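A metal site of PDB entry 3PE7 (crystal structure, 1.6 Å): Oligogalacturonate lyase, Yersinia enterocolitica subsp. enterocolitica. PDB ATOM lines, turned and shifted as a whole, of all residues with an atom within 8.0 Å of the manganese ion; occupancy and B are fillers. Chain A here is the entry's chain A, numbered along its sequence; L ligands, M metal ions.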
ATOM      1  N   TYR A  37     -12.494  18.338  -6.762  1.00  0.00           N
ATOM      2  CA  TYR A  37     -11.950  19.588  -7.277  1.00  0.00           C
ATOM      3  C   TYR A  37     -13.066  20.423  -7.935  1.00  0.00           C
ATOM      4  O   TYR A  37     -13.970  19.882  -8.590  1.00  0.00           O
ATOM      5  CB  TYR A  37     -10.797  19.335  -8.259  1.00  0.00           C
ATOM      6  CG  TYR A  37      -9.505  18.887  -7.607  1.00  0.00           C
ATOM      7  CD1 TYR A  37      -9.102  19.406  -6.374  1.00  0.00           C
ATOM      8  CD2 TYR A  37      -8.651  17.997  -8.262  1.00  0.00           C
ATOM      9  CE1 TYR A  37      -7.870  19.005  -5.787  1.00  0.00           C
ATOM     10  CE2 TYR A  37      -7.446  17.612  -7.701  1.00  0.00           C
ATOM     11  CZ  TYR A  37      -7.065  18.108  -6.475  1.00  0.00           C
ATOM     12  OH  TYR A  37      -5.861  17.692  -5.932  1.00  0.00           O
ATOM     13  N   PHE A  38     -13.007  21.734  -7.724  1.00  0.00           N
ATOM     14  CA  PHE A  38     -14.130  22.635  -8.031  1.00  0.00           C
ATOM     15  C   PHE A  38     -14.493  22.731  -9.506  1.00  0.00           C
ATOM     16  O   PHE A  38     -15.625  23.105  -9.834  1.00  0.00           O
ATOM     17  CB  PHE A  38     -13.849  24.055  -7.479  1.00  0.00           C
ATOM     18  CG  PHE A  38     -12.609  24.681  -8.014  1.00  0.00           C
ATOM     19  CD1 PHE A  38     -12.612  25.398  -9.209  1.00  0.00           C
ATOM     20  CD2 PHE A  38     -11.398  24.520  -7.318  1.00  0.00           C
ATOM     21  CE1 PHE A  38     -11.440  25.966  -9.723  1.00  0.00           C
ATOM     22  CE2 PHE A  38     -10.222  25.072  -7.832  1.00  0.00           C
ATOM     23  CZ  PHE A  38     -10.245  25.796  -9.015  1.00  0.00           C
ATOM     24  N   TYR A  39     -13.545  22.428 -10.381  1.00  0.00           N
ATOM     25  CA  TYR A  39     -13.792  22.523 -11.836  1.00  0.00           C
ATOM     26  C   TYR A  39     -14.363  21.232 -12.443  1.00  0.00           C
ATOM     27  O   TYR A  39     -14.753  21.212 -13.645  1.00  0.00           O
ATOM     28  CB  TYR A  39     -12.528  22.988 -12.576  1.00  0.00           C
ATOM     29  CG  TYR A  39     -11.301  22.141 -12.282  1.00  0.00           C
ATOM     30  CD1 TYR A  39     -10.475  22.415 -11.190  1.00  0.00           C
ATOM     31  CD2 TYR A  39     -10.990  21.040 -13.099  1.00  0.00           C
ATOM     32  CE1 TYR A  39      -9.346  21.621 -10.917  1.00  0.00           C
ATOM     33  CE2 TYR A  39      -9.891  20.255 -12.836  1.00  0.00           C
ATOM     34  CZ  TYR A  39      -9.076  20.538 -11.743  1.00  0.00           C
ATOM     35  OH  TYR A  39      -7.970  19.743 -11.495  1.00  0.00           O
ATOM     36  N   PHE A  84     -10.272  13.211  -5.430  1.00  0.00           N
ATOM     37  CA  PHE A  84     -10.375  14.623  -5.779  1.00  0.00           C
ATOM     38  C   PHE A  84     -10.627  14.853  -7.254  1.00  0.00           C
ATOM     39  O   PHE A  84     -11.390  15.748  -7.627  1.00  0.00           O
ATOM     40  CB  PHE A  84      -9.093  15.380  -5.356  1.00  0.00           C
ATOM     41  CG  PHE A  84      -8.948  15.464  -3.870  1.00  0.00           C
ATOM     42  CD1 PHE A  84      -8.442  14.379  -3.139  1.00  0.00           C
ATOM     43  CD2 PHE A  84      -9.332  16.618  -3.181  1.00  0.00           C
ATOM     44  CE1 PHE A  84      -8.324  14.457  -1.756  1.00  0.00           C
ATOM     45  CE2 PHE A  84      -9.216  16.695  -1.812  1.00  0.00           C
ATOM     46  CZ  PHE A  84      -8.713  15.620  -1.104  1.00  0.00           C
ATOM     47  N   TRP A 155       5.821  20.860   0.232  1.00  0.00           N
ATOM     48  CA  TRP A 155       6.034  22.048  -0.607  1.00  0.00           C
ATOM     49  C   TRP A 155       7.478  22.332  -1.002  1.00  0.00           C
ATOM     50  O   TRP A 155       7.717  22.937  -2.046  1.00  0.00           O
ATOM     51  CB  TRP A 155       5.340  23.271  -0.007  1.00  0.00           C
ATOM     52  CG  TRP A 155       3.854  23.104  -0.080  1.00  0.00           C
ATOM     53  CD1 TRP A 155       2.998  22.813   0.942  1.00  0.00           C
ATOM     54  CD2 TRP A 155       3.054  23.146  -1.270  1.00  0.00           C
ATOM     55  NE1 TRP A 155       1.709  22.701   0.473  1.00  0.00           N
ATOM     56  CE2 TRP A 155       1.711  22.891  -0.884  1.00  0.00           C
ATOM     57  CE3 TRP A 155       3.335  23.392  -2.632  1.00  0.00           C
ATOM     58  CZ2 TRP A 155       0.651  22.886  -1.797  1.00  0.00           C
ATOM     59  CZ3 TRP A 155       2.275  23.375  -3.536  1.00  0.00           C
ATOM     60  CH2 TRP A 155       0.945  23.120  -3.117  1.00  0.00           C
ATOM     61  N   SER A 286      -7.769  31.472  -2.201  1.00  0.00           N
ATOM     62  CA  SER A 286      -6.913  30.332  -2.539  1.00  0.00           C
ATOM     63  C   SER A 286      -7.324  29.665  -3.842  1.00  0.00           C
ATOM     64  O   SER A 286      -6.550  28.944  -4.433  1.00  0.00           O
ATOM     65  CB  SER A 286      -6.907  29.329  -1.387  1.00  0.00           C
ATOM     66  OG  SER A 286      -6.156  29.870  -0.301  1.00  0.00           O
ATOM     67  N   HIS A 287      -8.564  29.907  -4.250  1.00  0.00           N
ATOM     68  CA  HIS A 287      -9.160  29.343  -5.467  1.00  0.00           C
ATOM     69  C   HIS A 287     -10.179  30.344  -6.010  1.00  0.00           C
ATOM     70  O   HIS A 287     -10.580  31.287  -5.309  1.00  0.00           O
ATOM     71  CB  HIS A 287      -9.854  28.026  -5.168  1.00  0.00           C
ATOM     72  CG  HIS A 287      -8.993  27.057  -4.422  1.00  0.00           C
ATOM     73  ND1 HIS A 287      -8.969  26.999  -3.041  1.00  0.00           N
ATOM     74  CD2 HIS A 287      -8.100  26.141  -4.864  1.00  0.00           C
ATOM     75  CE1 HIS A 287      -8.097  26.066  -2.664  1.00  0.00           C
ATOM     76  NE2 HIS A 287      -7.563  25.531  -3.756  1.00  0.00           N
ATOM     77  N   ASP A 300     -12.432  31.513  -1.959  1.00  0.00           N
ATOM     78  CA  ASP A 300     -12.263  31.177  -0.542  1.00  0.00           C
ATOM     79  C   ASP A 300     -11.135  31.972   0.069  1.00  0.00           C
ATOM     80  O   ASP A 300      -9.975  31.825  -0.330  1.00  0.00           O
ATOM     81  CB  ASP A 300     -12.085  29.651  -0.313  1.00  0.00           C
ATOM     82  CG  ASP A 300     -11.129  28.968  -1.309  1.00  0.00           C
ATOM     83  OD1 ASP A 300     -10.868  27.759  -1.095  1.00  0.00           O
ATOM     84  OD2 ASP A 300     -10.688  29.570  -2.315  1.00  0.00           O
ATOM     85  N   TRP A 342      -7.092  24.747   7.159  1.00  0.00           N
ATOM     86  CA  TRP A 342      -6.077  24.463   6.129  1.00  0.00           C
ATOM     87  C   TRP A 342      -5.093  23.336   6.504  1.00  0.00           C
ATOM     88  O   TRP A 342      -4.081  23.125   5.809  1.00  0.00           O
ATOM     89  CB  TRP A 342      -5.308  25.734   5.754  1.00  0.00           C
ATOM     90  CG  TRP A 342      -6.198  26.849   5.289  1.00  0.00           C
ATOM     91  CD1 TRP A 342      -6.652  27.918   6.030  1.00  0.00           C
ATOM     92  CD2 TRP A 342      -6.717  27.040   3.960  1.00  0.00           C
ATOM     93  NE1 TRP A 342      -7.430  28.739   5.261  1.00  0.00           N
ATOM     94  CE2 TRP A 342      -7.479  28.237   3.982  1.00  0.00           C
ATOM     95  CE3 TRP A 342      -6.631  26.308   2.757  1.00  0.00           C
ATOM     96  CZ2 TRP A 342      -8.156  28.705   2.852  1.00  0.00           C
ATOM     97  CZ3 TRP A 342      -7.299  26.796   1.631  1.00  0.00           C
ATOM     98  CH2 TRP A 342      -8.062  27.977   1.691  1.00  0.00           C
ATOM     99  N   ARG A 349      -2.812  17.418   1.250  1.00  0.00           N
ATOM    100  CA  ARG A 349      -2.693  18.862   1.353  1.00  0.00           C
ATOM    101  C   ARG A 349      -3.854  19.596   0.680  1.00  0.00           C
ATOM    102  O   ARG A 349      -3.848  20.822   0.671  1.00  0.00           O
ATOM    103  CB  ARG A 349      -1.381  19.357   0.724  1.00  0.00           C
ATOM    104  CG  ARG A 349      -0.128  18.562   1.087  1.00  0.00           C
ATOM    105  CD  ARG A 349       0.090  18.508   2.550  1.00  0.00           C
ATOM    106  NE  ARG A 349       1.367  17.917   2.937  1.00  0.00           N
ATOM    107  CZ  ARG A 349       2.364  18.606   3.492  1.00  0.00           C
ATOM    108  NH1 ARG A 349       2.248  19.912   3.724  1.00  0.00           N
ATOM    109  NH2 ARG A 349       3.483  17.974   3.829  1.00  0.00           N
ATOM    110  N   GLN A 350      -4.819  18.868   0.130  1.00  0.00           N
ATOM    111  CA  GLN A 350      -5.984  19.519  -0.511  1.00  0.00           C
ATOM    112  C   GLN A 350      -7.257  19.304   0.269  1.00  0.00           C
ATOM    113  O   GLN A 350      -8.255  19.995   0.031  1.00  0.00           O
ATOM    114  CB  GLN A 350      -6.186  18.972  -1.943  1.00  0.00           C
ATOM    115  CG  GLN A 350      -5.123  19.408  -2.965  1.00  0.00           C
ATOM    116  CD  GLN A 350      -5.143  20.885  -3.265  1.00  0.00           C
ATOM    117  OE1 GLN A 350      -6.218  21.481  -3.498  1.00  0.00           O
ATOM    118  NE2 GLN A 350      -3.959  21.503  -3.286  1.00  0.00           N
ATOM    119  N   VAL A 351      -7.242  18.338   1.197  1.00  0.00           N
ATOM    120  CA  VAL A 351      -8.495  17.868   1.812  1.00  0.00           C
ATOM    121  C   VAL A 351      -9.274  18.966   2.567  1.00  0.00           C
ATOM    122  O   VAL A 351     -10.503  18.972   2.553  1.00  0.00           O
ATOM    123  CB  VAL A 351      -8.241  16.615   2.656  1.00  0.00           C
ATOM    124  CG1 VAL A 351      -7.477  16.945   3.944  1.00  0.00           C
ATOM    125  CG2 VAL A 351      -9.547  15.901   2.967  1.00  0.00           C
ATOM    126  N   THR A 352      -8.558  19.907   3.197  1.00  0.00           N
ATOM    127  CA  THR A 352      -9.246  20.995   3.912  1.00  0.00           C
ATOM    128  C   THR A 352      -9.456  22.234   3.060  1.00  0.00           C
ATOM    129  O   THR A 352      -9.959  23.236   3.558  1.00  0.00           O
ATOM    130  CB  THR A 352      -8.483  21.420   5.197  1.00  0.00           C
ATOM    131  OG1 THR A 352      -7.097  21.618   4.889  1.00  0.00           O
ATOM    132  CG2 THR A 352      -8.617  20.331   6.286  1.00  0.00           C
ATOM    133  N   HIS A 353      -9.086  22.178   1.763  1.00  0.00           N
ATOM    134  CA  HIS A 353      -9.367  23.313   0.857  1.00  0.00           C
ATOM    135  C   HIS A 353     -10.878  23.453   0.639  1.00  0.00           C
ATOM    136  O   HIS A 353     -11.536  22.490   0.298  1.00  0.00           O
ATOM    137  CB  HIS A 353      -8.656  23.111  -0.481  1.00  0.00           C
ATOM    138  CG  HIS A 353      -7.180  23.352  -0.414  1.00  0.00           C
ATOM    139  ND1 HIS A 353      -6.417  23.616  -1.529  1.00  0.00           N
ATOM    140  CD2 HIS A 353      -6.328  23.363   0.643  1.00  0.00           C
ATOM    141  CE1 HIS A 353      -5.161  23.798  -1.155  1.00  0.00           C
ATOM    142  NE2 HIS A 353      -5.084  23.659   0.150  1.00  0.00           N
ATOM    143  N   PRO A 354     -11.423  24.666   0.854  1.00  0.00           N
ATOM    144  CA  PRO A 354     -12.879  24.792   0.663  1.00  0.00           C
ATOM    145  C   PRO A 354     -13.335  24.481  -0.763  1.00  0.00           C
ATOM    146  O   PRO A 354     -14.366  23.847  -0.946  1.00  0.00           O
ATOM    147  CB  PRO A 354     -13.159  26.257   1.043  1.00  0.00           C
ATOM    148  CG  PRO A 354     -12.050  26.578   2.072  1.00  0.00           C
ATOM    149  CD  PRO A 354     -10.843  25.840   1.552  1.00  0.00           C
ATOM    150  N   HIS A 355     -12.553  24.910  -1.762  1.00  0.00           N
ATOM    151  CA  HIS A 355     -12.826  24.590  -3.182  1.00  0.00           C
ATOM    152  C   HIS A 355     -14.278  24.925  -3.578  1.00  0.00           C
ATOM    153  O   HIS A 355     -15.001  24.060  -4.105  1.00  0.00           O
ATOM    154  CB  HIS A 355     -12.504  23.094  -3.451  1.00  0.00           C
ATOM    155  CG  HIS A 355     -11.046  22.793  -3.532  1.00  0.00           C
ATOM    156  ND1 HIS A 355     -10.534  21.529  -3.364  1.00  0.00           N
ATOM    157  CD2 HIS A 355      -9.970  23.600  -3.747  1.00  0.00           C
ATOM    158  CE1 HIS A 355      -9.216  21.554  -3.488  1.00  0.00           C
ATOM    159  NE2 HIS A 355      -8.847  22.808  -3.720  1.00  0.00           N
HETATM  160  C1  LIG L   1      -5.300  23.924  -5.526  1.00  0.00           C
HETATM  161  O1  LIG L   1      -4.882  24.200  -4.335  1.00  0.00           O
HETATM  162  O2  LIG L   1      -6.516  23.526  -5.681  1.00  0.00           O
HETATM  163  C2  LIG L   1      -4.389  24.041  -6.700  1.00  0.00           C
HETATM  164 MN    MN M   1      -6.869  23.518  -3.618  1.00  0.00          MN
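A ring nitrogen (NE2) of His 353 sits at hydrogen-bond distance from the backbone carbonyl oxygen (O) of Arg 349, at 3.1 Å. A ring nitrogen (ND1) of His 287 sits at hydrogen-bond distance from the side-chain carboxylate (OD1) of Asp 300, 2.8 Å away. The backbone NH (N) of His 355 lies within hydrogen-bond range of the side-chain carboxylate (OD1) of Asp 300 (3.4 Å).
The manganese ion is bound by an oxygen (O2) of the ligand (2.1 Å), a ring nitrogen (NE2) of His 355 (2.1 Å), a ring nitrogen (NE2) of His 287 (2.1 Å), a ring nitrogen (ND1) of His 353 (2.1 Å), the side-chain amide oxygen of Gln 350 (2.1 Å) and an oxygen (O1) of the ligand (2.2 Å). The manganese ion has six donor atoms within binding distance.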
